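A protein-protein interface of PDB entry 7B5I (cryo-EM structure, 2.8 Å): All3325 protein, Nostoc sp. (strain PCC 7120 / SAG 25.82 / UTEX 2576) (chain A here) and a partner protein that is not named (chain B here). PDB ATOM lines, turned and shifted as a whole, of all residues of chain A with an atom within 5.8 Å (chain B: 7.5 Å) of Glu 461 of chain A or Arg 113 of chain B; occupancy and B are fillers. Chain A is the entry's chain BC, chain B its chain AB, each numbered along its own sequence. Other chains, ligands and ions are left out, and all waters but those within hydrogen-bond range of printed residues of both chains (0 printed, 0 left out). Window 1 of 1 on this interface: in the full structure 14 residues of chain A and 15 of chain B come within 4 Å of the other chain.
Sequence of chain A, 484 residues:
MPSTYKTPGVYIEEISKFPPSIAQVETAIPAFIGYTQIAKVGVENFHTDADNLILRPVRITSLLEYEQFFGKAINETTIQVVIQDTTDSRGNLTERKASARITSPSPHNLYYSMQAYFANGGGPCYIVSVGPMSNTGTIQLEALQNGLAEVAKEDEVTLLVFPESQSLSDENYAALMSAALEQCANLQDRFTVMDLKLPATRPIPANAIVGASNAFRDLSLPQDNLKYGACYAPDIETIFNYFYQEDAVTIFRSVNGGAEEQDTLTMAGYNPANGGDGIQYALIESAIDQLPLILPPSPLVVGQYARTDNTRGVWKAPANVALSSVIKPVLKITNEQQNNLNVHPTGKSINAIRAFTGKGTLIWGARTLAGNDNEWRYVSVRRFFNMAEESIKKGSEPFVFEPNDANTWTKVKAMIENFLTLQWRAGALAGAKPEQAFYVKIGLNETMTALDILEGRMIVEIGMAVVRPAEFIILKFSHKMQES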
ATOM      1  N   TYR A 439      10.432 -18.973 -28.608  1.00  0.00           N
ATOM      2  CA  TYR A 439       9.259 -19.322 -27.813  1.00  0.00           C
ATOM      3  C   TYR A 439       8.617 -18.066 -27.244  1.00  0.00           C
ATOM      4  O   TYR A 439       9.283 -17.048 -27.031  1.00  0.00           O
ATOM      5  CB  TYR A 439       9.594 -20.308 -26.679  1.00  0.00           C
ATOM      6  CG  TYR A 439      10.367 -19.716 -25.525  1.00  0.00           C
ATOM      7  CD1 TYR A 439       9.711 -19.089 -24.478  1.00  0.00           C
ATOM      8  CD2 TYR A 439      11.748 -19.800 -25.475  1.00  0.00           C
ATOM      9  CE1 TYR A 439      10.404 -18.544 -23.430  1.00  0.00           C
ATOM     10  CE2 TYR A 439      12.450 -19.260 -24.423  1.00  0.00           C
ATOM     11  CZ  TYR A 439      11.772 -18.634 -23.404  1.00  0.00           C
ATOM     12  OH  TYR A 439      12.464 -18.092 -22.347  1.00  0.00           O
ATOM     13  N   VAL A 440       7.311 -18.163 -26.978  1.00  0.00           N
ATOM     14  CA  VAL A 440       6.481 -17.060 -26.501  1.00  0.00           C
ATOM     15  C   VAL A 440       5.645 -17.553 -25.326  1.00  0.00           C
ATOM     16  O   VAL A 440       4.987 -18.593 -25.428  1.00  0.00           O
ATOM     17  CB  VAL A 440       5.560 -16.525 -27.615  1.00  0.00           C
ATOM     18  CG1 VAL A 440       4.711 -15.377 -27.101  1.00  0.00           C
ATOM     19  CG2 VAL A 440       6.367 -16.107 -28.827  1.00  0.00           C
ATOM     20  N   LYS A 441       5.665 -16.809 -24.216  1.00  0.00           N
ATOM     21  CA  LYS A 441       4.928 -17.161 -23.004  1.00  0.00           C
ATOM     22  C   LYS A 441       4.081 -15.983 -22.537  1.00  0.00           C
ATOM     23  O   LYS A 441       4.623 -14.934 -22.171  1.00  0.00           O
ATOM     24  CB  LYS A 441       5.878 -17.582 -21.884  1.00  0.00           C
ATOM     25  CG  LYS A 441       6.481 -18.950 -22.054  1.00  0.00           C
ATOM     26  CD  LYS A 441       7.276 -19.334 -20.826  1.00  0.00           C
ATOM     27  CE  LYS A 441       6.370 -19.970 -19.793  1.00  0.00           C
ATOM     28  NZ  LYS A 441       7.118 -20.516 -18.631  1.00  0.00           N
ATOM     29  N   ILE A 442       2.758 -16.163 -22.546  1.00  0.00           N
ATOM     30  CA  ILE A 442       1.807 -15.177 -22.037  1.00  0.00           C
ATOM     31  C   ILE A 442       0.586 -15.851 -21.413  1.00  0.00           C
ATOM     32  O   ILE A 442      -0.163 -16.551 -22.101  1.00  0.00           O
ATOM     33  CB  ILE A 442       1.389 -14.189 -23.144  1.00  0.00           C
ATOM     34  CG1 ILE A 442       0.314 -13.244 -22.612  1.00  0.00           C
ATOM     35  CG2 ILE A 442       0.944 -14.907 -24.408  1.00  0.00           C
ATOM     36  CD1 ILE A 442       0.003 -12.094 -23.520  1.00  0.00           C
ATOM     37  N   GLU A 446       1.812 -18.705 -16.910  1.00  0.00           N
ATOM     38  CA  GLU A 446       3.086 -18.478 -17.578  1.00  0.00           C
ATOM     39  C   GLU A 446       3.819 -17.276 -17.000  1.00  0.00           C
ATOM     40  O   GLU A 446       4.968 -17.416 -16.572  1.00  0.00           O
ATOM     41  CB  GLU A 446       2.874 -18.291 -19.087  1.00  0.00           C
ATOM     42  CG  GLU A 446       2.610 -19.559 -19.876  1.00  0.00           C
ATOM     43  CD  GLU A 446       1.321 -20.236 -19.482  1.00  0.00           C
ATOM     44  OE1 GLU A 446       1.246 -21.477 -19.580  1.00  0.00           O
ATOM     45  OE2 GLU A 446       0.376 -19.520 -19.090  1.00  0.00           O
ATOM     46  N   THR A 447       3.191 -16.096 -16.963  1.00  0.00           N
ATOM     47  CA  THR A 447       3.887 -14.890 -16.531  1.00  0.00           C
ATOM     48  C   THR A 447       3.023 -13.937 -15.719  1.00  0.00           C
ATOM     49  O   THR A 447       3.482 -12.834 -15.413  1.00  0.00           O
ATOM     50  CB  THR A 447       4.438 -14.122 -17.737  1.00  0.00           C
ATOM     51  OG1 THR A 447       3.449 -14.081 -18.766  1.00  0.00           O
ATOM     52  CG2 THR A 447       5.698 -14.765 -18.272  1.00  0.00           C
ATOM     53  N   ILE A 459       1.941  -9.257 -19.353  1.00  0.00           N
ATOM     54  CA  ILE A 459       3.355  -9.597 -19.410  1.00  0.00           C
ATOM     55  C   ILE A 459       3.599 -10.716 -20.414  1.00  0.00           C
ATOM     56  O   ILE A 459       2.963 -11.768 -20.357  1.00  0.00           O
ATOM     57  CB  ILE A 459       3.888 -10.029 -18.031  1.00  0.00           C
ATOM     58  CG1 ILE A 459       3.603  -8.947 -16.987  1.00  0.00           C
ATOM     59  CG2 ILE A 459       5.377 -10.326 -18.106  1.00  0.00           C
ATOM     60  CD1 ILE A 459       4.103  -9.289 -15.602  1.00  0.00           C
ATOM     61  N   VAL A 460       4.527 -10.475 -21.331  1.00  0.00           N
ATOM     62  CA  VAL A 460       4.867 -11.450 -22.366  1.00  0.00           C
ATOM     63  C   VAL A 460       6.372 -11.695 -22.332  1.00  0.00           C
ATOM     64  O   VAL A 460       7.155 -10.749 -22.198  1.00  0.00           O
ATOM     65  CB  VAL A 460       4.399 -10.985 -23.762  1.00  0.00           C
ATOM     66  CG1 VAL A 460       5.103  -9.706 -24.177  1.00  0.00           C
ATOM     67  CG2 VAL A 460       4.610 -12.065 -24.803  1.00  0.00           C
ATOM     68  N   GLU A 461       6.772 -12.963 -22.433  1.00  0.00           N
ATOM     69  CA  GLU A 461       8.178 -13.358 -22.453  1.00  0.00           C
ATOM     70  C   GLU A 461       8.522 -14.003 -23.791  1.00  0.00           C
ATOM     71  O   GLU A 461       7.844 -14.940 -24.217  1.00  0.00           O
ATOM     72  CB  GLU A 461       8.497 -14.310 -21.304  1.00  0.00           C
ATOM     73  CG  GLU A 461       8.395 -13.650 -19.946  1.00  0.00           C
ATOM     74  CD  GLU A 461       8.641 -14.614 -18.804  1.00  0.00           C
ATOM     75  OE1 GLU A 461       8.705 -15.832 -19.051  1.00  0.00           O
ATOM     76  OE2 GLU A 461       8.751 -14.151 -17.650  1.00  0.00           O
ATOM     77  N   ILE A 462       9.576 -13.515 -24.444  1.00  0.00           N
ATOM     78  CA  ILE A 462       9.945 -13.967 -25.784  1.00  0.00           C
ATOM     79  C   ILE A 462      11.417 -14.358 -25.809  1.00  0.00           C
ATOM     80  O   ILE A 462      12.285 -13.527 -25.519  1.00  0.00           O
ATOM     81  CB  ILE A 462       9.672 -12.884 -26.840  1.00  0.00           C
ATOM     82  CG1 ILE A 462       8.194 -12.507 -26.836  1.00  0.00           C
ATOM     83  CG2 ILE A 462      10.106 -13.371 -28.202  1.00  0.00           C
ATOM     84  CD1 ILE A 462       7.868 -11.300 -27.658  1.00  0.00           C
ATOM     85  N   GLY A 463      11.695 -15.606 -26.184  1.00  0.00           N
ATOM     86  CA  GLY A 463      13.057 -16.100 -26.328  1.00  0.00           C
ATOM     87  C   GLY A 463      13.395 -16.411 -27.775  1.00  0.00           C
ATOM     88  O   GLY A 463      12.568 -16.956 -28.509  1.00  0.00           O
ATOM     89  N   ILE B 110       1.954 -12.573  -5.205  1.00  0.00           N
ATOM     90  CA  ILE B 110       2.958 -11.563  -5.505  1.00  0.00           C
ATOM     91  C   ILE B 110       3.634 -11.917  -6.816  1.00  0.00           C
ATOM     92  O   ILE B 110       3.954 -13.084  -7.073  1.00  0.00           O
ATOM     93  CB  ILE B 110       3.981 -11.447  -4.365  1.00  0.00           C
ATOM     94  CG1 ILE B 110       3.272 -11.520  -3.013  1.00  0.00           C
ATOM     95  CG2 ILE B 110       4.775 -10.160  -4.500  1.00  0.00           C
ATOM     96  CD1 ILE B 110       4.152 -11.163  -1.842  1.00  0.00           C
ATOM     97  N   ASN B 111       3.853 -10.901  -7.653  1.00  0.00           N
ATOM     98  CA  ASN B 111       4.346 -11.116  -9.006  1.00  0.00           C
ATOM     99  C   ASN B 111       5.715 -11.773  -8.986  1.00  0.00           C
ATOM    100  O   ASN B 111       6.714 -11.156  -8.605  1.00  0.00           O
ATOM    101  CB  ASN B 111       4.407  -9.798  -9.777  1.00  0.00           C
ATOM    102  CG  ASN B 111       4.822  -9.991 -11.221  1.00  0.00           C
ATOM    103  OD1 ASN B 111       4.446 -10.975 -11.862  1.00  0.00           O
ATOM    104  ND2 ASN B 111       5.601  -9.050 -11.745  1.00  0.00           N
ATOM    105  N   SER B 112       5.758 -13.032  -9.402  1.00  0.00           N
ATOM    106  CA  SER B 112       6.993 -13.797  -9.464  1.00  0.00           C
ATOM    107  C   SER B 112       7.000 -14.568 -10.773  1.00  0.00           C
ATOM    108  O   SER B 112       6.319 -15.590 -10.901  1.00  0.00           O
ATOM    109  CB  SER B 112       7.115 -14.740  -8.272  1.00  0.00           C
ATOM    110  OG  SER B 112       8.329 -15.454  -8.335  1.00  0.00           O
ATOM    111  N   ARG B 113       7.760 -14.071 -11.741  1.00  0.00           N
ATOM    112  CA  ARG B 113       7.936 -14.736 -13.020  1.00  0.00           C
ATOM    113  C   ARG B 113       9.369 -15.194 -13.239  1.00  0.00           C
ATOM    114  O   ARG B 113       9.683 -15.703 -14.319  1.00  0.00           O
ATOM    115  CB  ARG B 113       7.501 -13.812 -14.166  1.00  0.00           C
ATOM    116  CG  ARG B 113       8.364 -12.576 -14.336  1.00  0.00           C
ATOM    117  CD  ARG B 113       7.781 -11.639 -15.387  1.00  0.00           C
ATOM    118  NE  ARG B 113       8.630 -10.472 -15.608  1.00  0.00           N
ATOM    119  CZ  ARG B 113       8.622  -9.380 -14.852  1.00  0.00           C
ATOM    120  NH1 ARG B 113       9.435  -8.376 -15.136  1.00  0.00           N
ATOM    121  NH2 ARG B 113       7.806  -9.291 -13.811  1.00  0.00           N
ATOM    122  N   ASN B 114      10.246 -15.009 -12.255  1.00  0.00           N
ATOM    123  CA  ASN B 114      11.628 -15.462 -12.321  1.00  0.00           C
ATOM    124  C   ASN B 114      11.930 -16.511 -11.257  1.00  0.00           C
ATOM    125  O   ASN B 114      13.081 -16.675 -10.850  1.00  0.00           O
ATOM    126  CB  ASN B 114      12.583 -14.280 -12.180  1.00  0.00           C
ATOM    127  CG  ASN B 114      12.084 -13.045 -12.894  1.00  0.00           C
ATOM    128  OD1 ASN B 114      12.328 -12.863 -14.085  1.00  0.00           O
ATOM    129  ND2 ASN B 114      11.383 -12.184 -12.165  1.00  0.00           N
ATOM    130  N   GLN B 115      10.909 -17.229 -10.799  1.00  0.00           N
ATOM    131  CA  GLN B 115      11.078 -18.212  -9.745  1.00  0.00           C
ATOM    132  C   GLN B 115      10.376 -19.498 -10.140  1.00  0.00           C
ATOM    133  O   GLN B 115       9.547 -19.523 -11.049  1.00  0.00           O
ATOM    134  CB  GLN B 115      10.529 -17.718  -8.405  1.00  0.00           C
ATOM    135  CG  GLN B 115      11.217 -16.488  -7.862  1.00  0.00           C
ATOM    136  CD  GLN B 115      10.646 -16.059  -6.534  1.00  0.00           C
ATOM    137  OE1 GLN B 115       9.743 -15.228  -6.477  1.00  0.00           O
ATOM    138  NE2 GLN B 115      11.169 -16.621  -5.454  1.00  0.00           N
ATOM    139  N   ILE B 116      10.714 -20.572  -9.427  1.00  0.00           N
ATOM    140  CA  ILE B 116      10.198 -21.901  -9.725  1.00  0.00           C
ATOM    141  C   ILE B 116      10.235 -22.715  -8.441  1.00  0.00           C
ATOM    142  O   ILE B 116      11.018 -22.439  -7.532  1.00  0.00           O
ATOM    143  CB  ILE B 116      11.014 -22.574 -10.858  1.00  0.00           C
ATOM    144  CG1 ILE B 116      10.377 -23.894 -11.294  1.00  0.00           C
ATOM    145  CG2 ILE B 116      12.454 -22.776 -10.430  1.00  0.00           C
ATOM    146  CD1 ILE B 116      11.132 -24.588 -12.383  1.00  0.00           C
ATOM    147  N   HIS B 190      10.188 -21.677  -3.087  1.00  0.00           N
ATOM    148  CA  HIS B 190      10.130 -20.766  -4.224  1.00  0.00           C
ATOM    149  C   HIS B 190      11.542 -20.247  -4.470  1.00  0.00           C
ATOM    150  O   HIS B 190      11.959 -19.234  -3.911  1.00  0.00           O
ATOM    151  CB  HIS B 190       9.137 -19.647  -3.944  1.00  0.00           C
ATOM    152  CG  HIS B 190       8.306 -19.263  -5.127  1.00  0.00           C
ATOM    153  ND1 HIS B 190       7.402 -18.224  -5.094  1.00  0.00           N
ATOM    154  CD2 HIS B 190       8.250 -19.771  -6.380  1.00  0.00           C
ATOM    155  CE1 HIS B 190       6.818 -18.115  -6.274  1.00  0.00           C
ATOM    156  NE2 HIS B 190       7.316 -19.041  -7.072  1.00  0.00           N
ATOM    157  N   ARG B 193      14.724 -18.940 -10.582  1.00  0.00           N
ATOM    158  CA  ARG B 193      15.146 -19.704 -11.744  1.00  0.00           C
ATOM    159  C   ARG B 193      16.049 -18.865 -12.638  1.00  0.00           C
ATOM    160  O   ARG B 193      15.914 -17.642 -12.720  1.00  0.00           O
ATOM    161  CB  ARG B 193      13.940 -20.208 -12.539  1.00  0.00           C
ATOM    162  CG  ARG B 193      13.388 -19.234 -13.558  1.00  0.00           C
ATOM    163  CD  ARG B 193      12.558 -19.961 -14.607  1.00  0.00           C
ATOM    164  NE  ARG B 193      11.208 -20.253 -14.134  1.00  0.00           N
ATOM    165  CZ  ARG B 193      10.339 -21.027 -14.774  1.00  0.00           C
ATOM    166  NH1 ARG B 193      10.677 -21.604 -15.917  1.00  0.00           N
ATOM    167  NH2 ARG B 193       9.133 -21.231 -14.267  1.00  0.00           N
ATOM    168  N   PRO B 274       9.984 -24.848 -21.482  1.00  0.00           N
ATOM    169  CA  PRO B 274       9.970 -23.562 -20.762  1.00  0.00           C
ATOM    170  C   PRO B 274       8.760 -23.346 -19.876  1.00  0.00           C
ATOM    171  O   PRO B 274       8.868 -22.612 -18.887  1.00  0.00           O
ATOM    172  CB  PRO B 274      10.022 -22.527 -21.895  1.00  0.00           C
ATOM    173  CG  PRO B 274       9.579 -23.245 -23.097  1.00  0.00           C
ATOM    174  CD  PRO B 274      10.034 -24.653 -22.939  1.00  0.00           C
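Printed residues of chain B within 4 Å of Lys 441 of chain A: Pro 274.
Of the printed residues of chain B, Ile 459 of chain A touches Arg 113 (3.9 Å).
Glu 461 of chain A touches just one residue of chain B: Arg 113 (3.5 Å).
Of the printed residues of chain A, Pro 274 of chain B touches Lys 441.
The nearest residue of chain B that does not touch Glu 461 of chain A is Asn 114 of chain B (5.2 Å).
The nearest printed residue of chain A that does not touch Pro 274 of chain B is Tyr 439 of chain A (4.3 Å).
Of the 11 printed residues of chain A, 3 touch a printed residue of chain B.
Among the printed residues, 3 pairs touch across the chains.
Among the printed residues, no Asp or Glu carboxylate lies within 4 Å of a Lys or Arg side-chain nitrogen of the other chain.
The backbone carbonyl oxygen of Pro 274 of chain B lies within hydrogen-bond range of the side-chain amino group of Lys 441 of chain A, at 2.7 Å.
Ile 459 of chain A touches Arg 113 of chain B.
Glu 461 of chain A touches Arg 113 of chain B (OE2 to CD, 3.5 Å).
The side-chain hydroxyl (OG1) of Thr 447 of chain A lies within hydrogen-bond range of the backbone carbonyl oxygen (O) of Ile 459 of chain A (2.8 Å).
ND2 of Asn 111 of chain B lies close to NH2 of Arg 113 of chain B, at 3.0 Å.
N of Lys 441 of chain A is in hydrogen-bond range of O of Glu 461 of chain A, 2.9 Å away.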
